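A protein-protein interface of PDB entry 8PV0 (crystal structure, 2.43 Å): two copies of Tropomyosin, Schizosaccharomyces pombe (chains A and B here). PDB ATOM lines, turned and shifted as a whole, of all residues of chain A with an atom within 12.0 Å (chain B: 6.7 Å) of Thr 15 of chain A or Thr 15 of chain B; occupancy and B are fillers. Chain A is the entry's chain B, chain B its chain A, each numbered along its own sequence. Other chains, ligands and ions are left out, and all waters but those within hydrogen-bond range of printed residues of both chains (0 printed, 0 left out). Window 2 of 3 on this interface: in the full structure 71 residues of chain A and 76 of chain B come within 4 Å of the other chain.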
ATOM      1  N   GLU A   6     -10.944 -32.053 -11.977  1.00  0.00           N
ATOM      2  CA  GLU A   6      -9.664 -31.580 -12.491  1.00  0.00           C
ATOM      3  C   GLU A   6      -9.362 -30.175 -11.993  1.00  0.00           C
ATOM      4  O   GLU A   6      -8.208 -29.846 -11.703  1.00  0.00           O
ATOM      5  CB  GLU A   6      -9.666 -31.616 -14.020  1.00  0.00           C
ATOM      6  CG  GLU A   6     -10.041 -32.963 -14.623  1.00  0.00           C
ATOM      7  CD  GLU A   6      -8.962 -34.017 -14.445  1.00  0.00           C
ATOM      8  OE1 GLU A   6      -8.778 -34.509 -13.312  1.00  0.00           O
ATOM      9  OE2 GLU A   6      -8.293 -34.354 -15.445  1.00  0.00           O
ATOM     10  N   LYS A   7     -10.392 -29.335 -11.874  1.00  0.00           N
ATOM     11  CA  LYS A   7     -10.196 -27.984 -11.359  1.00  0.00           C
ATOM     12  C   LYS A   7      -9.721 -28.004  -9.910  1.00  0.00           C
ATOM     13  O   LYS A   7      -8.787 -27.278  -9.545  1.00  0.00           O
ATOM     14  CB  LYS A   7     -11.497 -27.192 -11.491  1.00  0.00           C
ATOM     15  CG  LYS A   7     -11.429 -25.762 -10.985  1.00  0.00           C
ATOM     16  CD  LYS A   7     -12.731 -25.030 -11.256  1.00  0.00           C
ATOM     17  CE  LYS A   7     -12.700 -23.618 -10.703  1.00  0.00           C
ATOM     18  NZ  LYS A   7     -11.585 -22.817 -11.279  1.00  0.00           N
ATOM     19  N   ILE A   8     -10.352 -28.832  -9.073  1.00  0.00           N
ATOM     20  CA  ILE A   8      -9.939 -28.932  -7.675  1.00  0.00           C
ATOM     21  C   ILE A   8      -8.512 -29.456  -7.576  1.00  0.00           C
ATOM     22  O   ILE A   8      -7.699 -28.953  -6.786  1.00  0.00           O
ATOM     23  CB  ILE A   8     -10.921 -29.823  -6.893  1.00  0.00           C
ATOM     24  CG1 ILE A   8     -12.351 -29.295  -7.018  1.00  0.00           C
ATOM     25  CG2 ILE A   8     -10.516 -29.899  -5.433  1.00  0.00           C
ATOM     26  CD1 ILE A   8     -13.393 -30.263  -6.510  1.00  0.00           C
ATOM     27  N   ASN A   9      -8.186 -30.478  -8.372  1.00  0.00           N
ATOM     28  CA  ASN A   9      -6.834 -31.026  -8.347  1.00  0.00           C
ATOM     29  C   ASN A   9      -5.811 -29.995  -8.808  1.00  0.00           C
ATOM     30  O   ASN A   9      -4.710 -29.913  -8.253  1.00  0.00           O
ATOM     31  CB  ASN A   9      -6.760 -32.287  -9.207  1.00  0.00           C
ATOM     32  CG  ASN A   9      -7.537 -33.444  -8.609  1.00  0.00           C
ATOM     33  OD1 ASN A   9      -8.368 -34.059  -9.275  1.00  0.00           O
ATOM     34  ND2 ASN A   9      -7.269 -33.744  -7.343  1.00  0.00           N
ATOM     35  N   ALA A  10      -6.162 -29.186  -9.809  1.00  0.00           N
ATOM     36  CA  ALA A  10      -5.250 -28.151 -10.283  1.00  0.00           C
ATOM     37  C   ALA A  10      -5.042 -27.070  -9.228  1.00  0.00           C
ATOM     38  O   ALA A  10      -3.924 -26.570  -9.056  1.00  0.00           O
ATOM     39  CB  ALA A  10      -5.779 -27.545 -11.583  1.00  0.00           C
ATOM     40  N   ALA A  11      -6.105 -26.699  -8.512  1.00  0.00           N
ATOM     41  CA  ALA A  11      -5.966 -25.723  -7.434  1.00  0.00           C
ATOM     42  C   ALA A  11      -5.051 -26.253  -6.335  1.00  0.00           C
ATOM     43  O   ALA A  11      -4.165 -25.539  -5.838  1.00  0.00           O
ATOM     44  CB  ALA A  11      -7.345 -25.364  -6.873  1.00  0.00           C
ATOM     45  N   ARG A  12      -5.246 -27.517  -5.947  1.00  0.00           N
ATOM     46  CA  ARG A  12      -4.380 -28.114  -4.933  1.00  0.00           C
ATOM     47  C   ARG A  12      -2.932 -28.178  -5.407  1.00  0.00           C
ATOM     48  O   ARG A  12      -2.005 -27.906  -4.632  1.00  0.00           O
ATOM     49  CB  ARG A  12      -4.881 -29.509  -4.561  1.00  0.00           C
ATOM     50  CG  ARG A  12      -6.001 -29.510  -3.542  1.00  0.00           C
ATOM     51  CD  ARG A  12      -6.152 -30.878  -2.897  1.00  0.00           C
ATOM     52  NE  ARG A  12      -7.125 -30.861  -1.811  1.00  0.00           N
ATOM     53  CZ  ARG A  12      -8.398 -31.205  -1.942  1.00  0.00           C
ATOM     54  NH1 ARG A  12      -8.887 -31.613  -3.101  1.00  0.00           N
ATOM     55  NH2 ARG A  12      -9.199 -31.144  -0.882  1.00  0.00           N
ATOM     56  N   ALA A  13      -2.718 -28.540  -6.675  1.00  0.00           N
ATOM     57  CA  ALA A  13      -1.362 -28.603  -7.209  1.00  0.00           C
ATOM     58  C   ALA A  13      -0.709 -27.229  -7.215  1.00  0.00           C
ATOM     59  O   ALA A  13       0.479 -27.098  -6.904  1.00  0.00           O
ATOM     60  CB  ALA A  13      -1.377 -29.195  -8.618  1.00  0.00           C
ATOM     61  N   GLU A  14      -1.472 -26.191  -7.566  1.00  0.00           N
ATOM     62  CA  GLU A  14      -0.938 -24.833  -7.547  1.00  0.00           C
ATOM     63  C   GLU A  14      -0.513 -24.432  -6.140  1.00  0.00           C
ATOM     64  O   GLU A  14       0.584 -23.892  -5.937  1.00  0.00           O
ATOM     65  CB  GLU A  14      -1.980 -23.861  -8.098  1.00  0.00           C
ATOM     66  CG  GLU A  14      -1.574 -22.402  -8.025  1.00  0.00           C
ATOM     67  CD  GLU A  14      -2.614 -21.482  -8.633  1.00  0.00           C
ATOM     68  OE1 GLU A  14      -3.557 -21.992  -9.274  1.00  0.00           O
ATOM     69  OE2 GLU A  14      -2.491 -20.251  -8.469  1.00  0.00           O
ATOM     70  N   THR A  15      -1.373 -24.692  -5.151  1.00  0.00           N
ATOM     71  CA  THR A  15      -1.028 -24.358  -3.770  1.00  0.00           C
ATOM     72  C   THR A  15       0.220 -25.109  -3.310  1.00  0.00           C
ATOM     73  O   THR A  15       1.128 -24.519  -2.702  1.00  0.00           O
ATOM     74  CB  THR A  15      -2.212 -24.663  -2.851  1.00  0.00           C
ATOM     75  OG1 THR A  15      -3.306 -23.795  -3.176  1.00  0.00           O
ATOM     76  CG2 THR A  15      -1.831 -24.466  -1.392  1.00  0.00           C
ATOM     77  N   ASP A  16       0.287 -26.413  -3.599  1.00  0.00           N
ATOM     78  CA  ASP A  16       1.433 -27.212  -3.176  1.00  0.00           C
ATOM     79  C   ASP A  16       2.718 -26.738  -3.844  1.00  0.00           C
ATOM     80  O   ASP A  16       3.773 -26.679  -3.201  1.00  0.00           O
ATOM     81  CB  ASP A  16       1.183 -28.688  -3.480  1.00  0.00           C
ATOM     82  CG  ASP A  16       0.037 -29.265  -2.671  1.00  0.00           C
ATOM     83  OD1 ASP A  16      -0.180 -28.803  -1.530  1.00  0.00           O
ATOM     84  OD2 ASP A  16      -0.645 -30.179  -3.176  1.00  0.00           O
ATOM     85  N   GLU A  17       2.652 -26.397  -5.133  1.00  0.00           N
ATOM     86  CA  GLU A  17       3.842 -25.926  -5.831  1.00  0.00           C
ATOM     87  C   GLU A  17       4.292 -24.573  -5.303  1.00  0.00           C
ATOM     88  O   GLU A  17       5.496 -24.310  -5.213  1.00  0.00           O
ATOM     89  CB  GLU A  17       3.579 -25.868  -7.335  1.00  0.00           C
ATOM     90  CG  GLU A  17       3.693 -27.221  -8.018  1.00  0.00           C
ATOM     91  CD  GLU A  17       2.667 -27.414  -9.115  1.00  0.00           C
ATOM     92  OE1 GLU A  17       2.089 -26.408  -9.577  1.00  0.00           O
ATOM     93  OE2 GLU A  17       2.432 -28.576  -9.508  1.00  0.00           O
ATOM     94  N   ALA A  18       3.346 -23.709  -4.925  1.00  0.00           N
ATOM     95  CA  ALA A  18       3.723 -22.436  -4.317  1.00  0.00           C
ATOM     96  C   ALA A  18       4.450 -22.655  -2.995  1.00  0.00           C
ATOM     97  O   ALA A  18       5.505 -22.052  -2.741  1.00  0.00           O
ATOM     98  CB  ALA A  18       2.485 -21.563  -4.114  1.00  0.00           C
ATOM     99  N   VAL A  19       3.899 -23.521  -2.138  1.00  0.00           N
ATOM    100  CA  VAL A  19       4.538 -23.790  -0.850  1.00  0.00           C
ATOM    101  C   VAL A  19       5.931 -24.380  -1.054  1.00  0.00           C
ATOM    102  O   VAL A  19       6.899 -23.981  -0.387  1.00  0.00           O
ATOM    103  CB  VAL A  19       3.655 -24.717   0.005  1.00  0.00           C
ATOM    104  CG1 VAL A  19       4.375 -25.095   1.291  1.00  0.00           C
ATOM    105  CG2 VAL A  19       2.327 -24.045   0.313  1.00  0.00           C
ATOM    106  N   ALA A  20       6.052 -25.342  -1.974  1.00  0.00           N
ATOM    107  CA  ALA A  20       7.343 -25.969  -2.228  1.00  0.00           C
ATOM    108  C   ALA A  20       8.352 -24.963  -2.763  1.00  0.00           C
ATOM    109  O   ALA A  20       9.520 -24.976  -2.357  1.00  0.00           O
ATOM    110  CB  ALA A  20       7.179 -27.135  -3.203  1.00  0.00           C
ATOM    111  N   ARG A  21       7.925 -24.089  -3.679  1.00  0.00           N
ATOM    112  CA  ARG A  21       8.824 -23.064  -4.193  1.00  0.00           C
ATOM    113  C   ARG A  21       9.314 -22.158  -3.075  1.00  0.00           C
ATOM    114  O   ARG A  21      10.511 -21.860  -2.993  1.00  0.00           O
ATOM    115  CB  ARG A  21       8.131 -22.249  -5.285  1.00  0.00           C
ATOM    116  CG  ARG A  21       9.025 -21.191  -5.922  1.00  0.00           C
ATOM    117  CD  ARG A  21       8.500 -20.750  -7.280  1.00  0.00           C
ATOM    118  NE  ARG A  21       7.269 -19.974  -7.184  1.00  0.00           N
ATOM    119  CZ  ARG A  21       7.209 -18.651  -7.252  1.00  0.00           C
ATOM    120  NH1 ARG A  21       8.298 -17.917  -7.415  1.00  0.00           N
ATOM    121  NH2 ARG A  21       6.028 -18.049  -7.155  1.00  0.00           N
ATOM    122  N   ALA A  22       8.407 -21.725  -2.196  1.00  0.00           N
ATOM    123  CA  ALA A  22       8.805 -20.870  -1.080  1.00  0.00           C
ATOM    124  C   ALA A  22       9.846 -21.557  -0.200  1.00  0.00           C
ATOM    125  O   ALA A  22      10.901 -20.978   0.112  1.00  0.00           O
ATOM    126  CB  ALA A  22       7.575 -20.481  -0.260  1.00  0.00           C
ATOM    127  N   GLU A  23       9.571 -22.801   0.200  1.00  0.00           N
ATOM    128  CA  GLU A  23      10.474 -23.503   1.109  1.00  0.00           C
ATOM    129  C   GLU A  23      11.837 -23.743   0.464  1.00  0.00           C
ATOM    130  O   GLU A  23      12.884 -23.522   1.093  1.00  0.00           O
ATOM    131  CB  GLU A  23       9.840 -24.821   1.559  1.00  0.00           C
ATOM    132  CG  GLU A  23       8.570 -24.646   2.386  1.00  0.00           C
ATOM    133  CD  GLU A  23       7.919 -25.966   2.761  1.00  0.00           C
ATOM    134  OE1 GLU A  23       8.333 -27.013   2.216  1.00  0.00           O
ATOM    135  OE2 GLU A  23       6.996 -25.956   3.603  1.00  0.00           O
ATOM    136  N   ALA A  24      11.842 -24.187  -0.798  1.00  0.00           N
ATOM    137  CA  ALA A  24      13.100 -24.438  -1.492  1.00  0.00           C
ATOM    138  C   ALA A  24      13.902 -23.157  -1.658  1.00  0.00           C
ATOM    139  O   ALA A  24      15.128 -23.160  -1.496  1.00  0.00           O
ATOM    140  CB  ALA A  24      12.830 -25.082  -2.851  1.00  0.00           C
ATOM    141  N   GLU A  26      13.859 -20.479   0.290  1.00  0.00           N
ATOM    142  CA  GLU A  26      14.431 -20.072   1.573  1.00  0.00           C
ATOM    143  C   GLU A  26      15.636 -20.937   1.941  1.00  0.00           C
ATOM    144  O   GLU A  26      16.678 -20.426   2.390  1.00  0.00           O
ATOM    145  CB  GLU A  26      13.361 -20.128   2.664  1.00  0.00           C
ATOM    146  CG  GLU A  26      12.257 -19.104   2.479  1.00  0.00           C
ATOM    147  CD  GLU A  26      11.192 -19.202   3.550  1.00  0.00           C
ATOM    148  OE1 GLU A  26      11.226 -20.176   4.331  1.00  0.00           O
ATOM    149  OE2 GLU A  26      10.326 -18.304   3.611  1.00  0.00           O
ATOM    150  N   ALA B  10      -9.288 -19.711   2.634  1.00  0.00           N
ATOM    151  CA  ALA B  10      -8.065 -20.051   3.351  1.00  0.00           C
ATOM    152  C   ALA B  10      -7.001 -20.587   2.400  1.00  0.00           C
ATOM    153  O   ALA B  10      -5.815 -20.259   2.531  1.00  0.00           O
ATOM    154  CB  ALA B  10      -8.370 -21.066   4.453  1.00  0.00           C
ATOM    155  N   ALA B  11      -7.412 -21.403   1.425  1.00  0.00           N
ATOM    156  CA  ALA B  11      -6.468 -21.921   0.442  1.00  0.00           C
ATOM    157  C   ALA B  11      -5.898 -20.800  -0.418  1.00  0.00           C
ATOM    158  O   ALA B  11      -4.698 -20.788  -0.720  1.00  0.00           O
ATOM    159  CB  ALA B  11      -7.145 -22.978  -0.431  1.00  0.00           C
ATOM    160  N   ARG B  12      -6.744 -19.848  -0.823  1.00  0.00           N
ATOM    161  CA  ARG B  12      -6.252 -18.730  -1.626  1.00  0.00           C
ATOM    162  C   ARG B  12      -5.276 -17.872  -0.829  1.00  0.00           C
ATOM    163  O   ARG B  12      -4.261 -17.413  -1.367  1.00  0.00           O
ATOM    164  CB  ARG B  12      -7.425 -17.894  -2.155  1.00  0.00           C
ATOM    165  CG  ARG B  12      -7.843 -16.709  -1.284  1.00  0.00           C
ATOM    166  CD  ARG B  12      -9.157 -16.085  -1.736  1.00  0.00           C
ATOM    167  NE  ARG B  12      -9.616 -15.069  -0.794  1.00  0.00           N
ATOM    168  CZ  ARG B  12     -10.744 -14.383  -0.916  1.00  0.00           C
ATOM    169  NH1 ARG B  12     -11.562 -14.572  -1.939  1.00  0.00           N
ATOM    170  NH2 ARG B  12     -11.061 -13.484   0.012  1.00  0.00           N
ATOM    171  N   ALA B  13      -5.547 -17.675   0.466  1.00  0.00           N
ATOM    172  CA  ALA B  13      -4.646 -16.883   1.296  1.00  0.00           C
ATOM    173  C   ALA B  13      -3.313 -17.597   1.483  1.00  0.00           C
ATOM    174  O   ALA B  13      -2.245 -16.977   1.395  1.00  0.00           O
ATOM    175  CB  ALA B  13      -5.300 -16.588   2.647  1.00  0.00           C
ATOM    176  N   GLU B  14      -3.361 -18.907   1.739  1.00  0.00           N
ATOM    177  CA  GLU B  14      -2.139 -19.695   1.848  1.00  0.00           C
ATOM    178  C   GLU B  14      -1.325 -19.637   0.559  1.00  0.00           C
ATOM    179  O   GLU B  14      -0.100 -19.467   0.596  1.00  0.00           O
ATOM    180  CB  GLU B  14      -2.496 -21.138   2.208  1.00  0.00           C
ATOM    181  CG  GLU B  14      -1.398 -22.161   1.974  1.00  0.00           C
ATOM    182  CD  GLU B  14      -1.884 -23.586   2.181  1.00  0.00           C
ATOM    183  OE1 GLU B  14      -3.027 -23.764   2.649  1.00  0.00           O
ATOM    184  OE2 GLU B  14      -1.124 -24.529   1.874  1.00  0.00           O
ATOM    185  N   THR B  15      -1.992 -19.754  -0.592  1.00  0.00           N
ATOM    186  CA  THR B  15      -1.282 -19.729  -1.866  1.00  0.00           C
ATOM    187  C   THR B  15      -0.633 -18.373  -2.106  1.00  0.00           C
ATOM    188  O   THR B  15       0.528 -18.294  -2.525  1.00  0.00           O
ATOM    189  CB  THR B  15      -2.242 -20.079  -3.004  1.00  0.00           C
ATOM    190  OG1 THR B  15      -2.840 -21.355  -2.746  1.00  0.00           O
ATOM    191  CG2 THR B  15      -1.504 -20.122  -4.339  1.00  0.00           C
ATOM    192  N   ASP B  16      -1.367 -17.291  -1.840  1.00  0.00           N
ATOM    193  CA  ASP B  16      -0.808 -15.961  -2.050  1.00  0.00           C
ATOM    194  C   ASP B  16       0.380 -15.710  -1.133  1.00  0.00           C
ATOM    195  O   ASP B  16       1.401 -15.156  -1.563  1.00  0.00           O
ATOM    196  CB  ASP B  16      -1.886 -14.903  -1.839  1.00  0.00           C
ATOM    197  CG  ASP B  16      -3.000 -14.997  -2.859  1.00  0.00           C
ATOM    198  OD1 ASP B  16      -2.909 -15.841  -3.777  1.00  0.00           O
ATOM    199  OD2 ASP B  16      -3.970 -14.222  -2.738  1.00  0.00           O
ATOM    200  N   GLU B  17       0.272 -16.118   0.134  1.00  0.00           N
ATOM    201  CA  GLU B  17       1.388 -15.940   1.056  1.00  0.00           C
ATOM    202  C   GLU B  17       2.604 -16.742   0.608  1.00  0.00           C
ATOM    203  O   GLU B  17       3.738 -16.246   0.659  1.00  0.00           O
ATOM    204  CB  GLU B  17       0.972 -16.340   2.470  1.00  0.00           C
ATOM    205  CG  GLU B  17       2.081 -16.183   3.497  1.00  0.00           C
ATOM    206  CD  GLU B  17       2.035 -17.248   4.574  1.00  0.00           C
ATOM    207  OE1 GLU B  17       1.235 -18.198   4.440  1.00  0.00           O
ATOM    208  OE2 GLU B  17       2.800 -17.137   5.555  1.00  0.00           O
ATOM    209  N   ALA B  18       2.387 -17.985   0.166  1.00  0.00           N
ATOM    210  CA  ALA B  18       3.502 -18.808  -0.291  1.00  0.00           C
ATOM    211  C   ALA B  18       4.173 -18.193  -1.511  1.00  0.00           C
ATOM    212  O   ALA B  18       5.405 -18.179  -1.607  1.00  0.00           O
ATOM    213  CB  ALA B  18       3.018 -20.226  -0.593  1.00  0.00           C
ATOM    214  N   VAL B  19       3.379 -17.661  -2.443  1.00  0.00           N
ATOM    215  CA  VAL B  19       3.944 -17.032  -3.635  1.00  0.00           C
ATOM    216  C   VAL B  19       4.758 -15.800  -3.255  1.00  0.00           C
ATOM    217  O   VAL B  19       5.857 -15.578  -3.782  1.00  0.00           O
ATOM    218  CB  VAL B  19       2.825 -16.690  -4.636  1.00  0.00           C
ATOM    219  CG1 VAL B  19       3.359 -15.810  -5.758  1.00  0.00           C
ATOM    220  CG2 VAL B  19       2.221 -17.962  -5.202  1.00  0.00           C
ATOM    221  N   ALA B  20       4.237 -14.985  -2.334  1.00  0.00           N
ATOM    222  CA  ALA B  20       4.955 -13.782  -1.921  1.00  0.00           C
ATOM    223  C   ALA B  20       6.282 -14.133  -1.257  1.00  0.00           C
ATOM    224  O   ALA B  20       7.326 -13.532  -1.560  1.00  0.00           O
ATOM    225  CB  ALA B  20       4.081 -12.951  -0.982  1.00  0.00           C
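OG1 of Thr 15 of chain B sits at hydrogen-bond distance from OG1 of Thr 15 of chain A, 2.5 Å away.
OG1 of Thr 15 of chain B is in hydrogen-bond range of O of Ala 11 of chain B. The backbone carbonyl oxygen (O) of Ala 11 of chain A is in hydrogen-bond range of the side-chain hydroxyl (OG1) of Thr 15 of chain A (3.3 Å).
Among the printed residues, pairs that only touch across the chains: Thr 15 of chain A with Glu 14 of chain B (3.3 Å), Ala 22 of chain A with Ala 18 of chain B (3.4 Å), Ala 18 of chain A with Ala 18 of chain B (3.7 Å), Val 19 of chain A with Ala 18 of chain B (3.7 Å), Arg 21 of chain A with Val 19 of chain B (3.8 Å), Ala 18 of chain A with Val 19 of chain B (3.8 Å) and Val 19 of chain A with Glu 14 of chain B (3.8 Å).
Thr 15 of chain A touches just these residues of chain B: Glu 14 (3.3 Å) and Thr 15 (2.5 Å). No residue of chain A comes within 4 Å of Ala 11 of chain B. Glu 14 of chain B touches just these residues of chain A: Thr 15 (3.3 Å) and Val 19 (3.8 Å). Asp 16 of chain B touches none of the printed residues of chain A. Ala 18 of chain B touches just these residues of chain A: Ala 18 (3.7 Å), Val 19 (3.7 Å) and Ala 22 (3.4 Å). Printed residues of chain B within 4 Å of Ala 22 of chain A: Ala 18. Printed residues of chain B within 4 Å of Ala 18 of chain A: Ala 18 (3.7 Å) and Val 19 (3.8 Å). Of the printed residues of chain B, Val 19 of chain A touches Glu 14 (3.8 Å) and Ala 18 (3.7 Å). Glu 23 of chain A touches none of the printed residues of chain B. Arg 12 of chain B touches none of the printed residues of chain A. The nearest printed residue of chain B that does not touch Ala 18 of chain A is Thr 15 of chain B (4.1 Å).
Printed residues of chain B that touch a printed residue of chain A: Glu 14, Thr 15, Ala 18 and Val 19. Of the 20 printed residues of chain A, 5 touch a printed residue of chain B. Among the printed residues, 8 pairs touch across the chains. Among the printed residues, no Asp or Glu carboxylate lies within 4 Å of a Lys or Arg side-chain nitrogen of the other chain.
Thr 15 of chain A touches Glu 14 of chain B, but with the chains exchanged Glu 14 of chain A does not touch Thr 15 of chain B (4.2 Å). Thr 15 of chain A touches its own counterpart, Thr 15 of chain B. Ala 18 of chain A touches its own counterpart, Ala 18 of chain B. Ala 18 of chain A touches Val 19 of chain B, and with the chains exchanged Val 19 of chain A touches Ala 18 of chain B. Of the 8 pairs that touch across the chains among the printed residues, 4 have their exchanged pair printed and touching as well.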
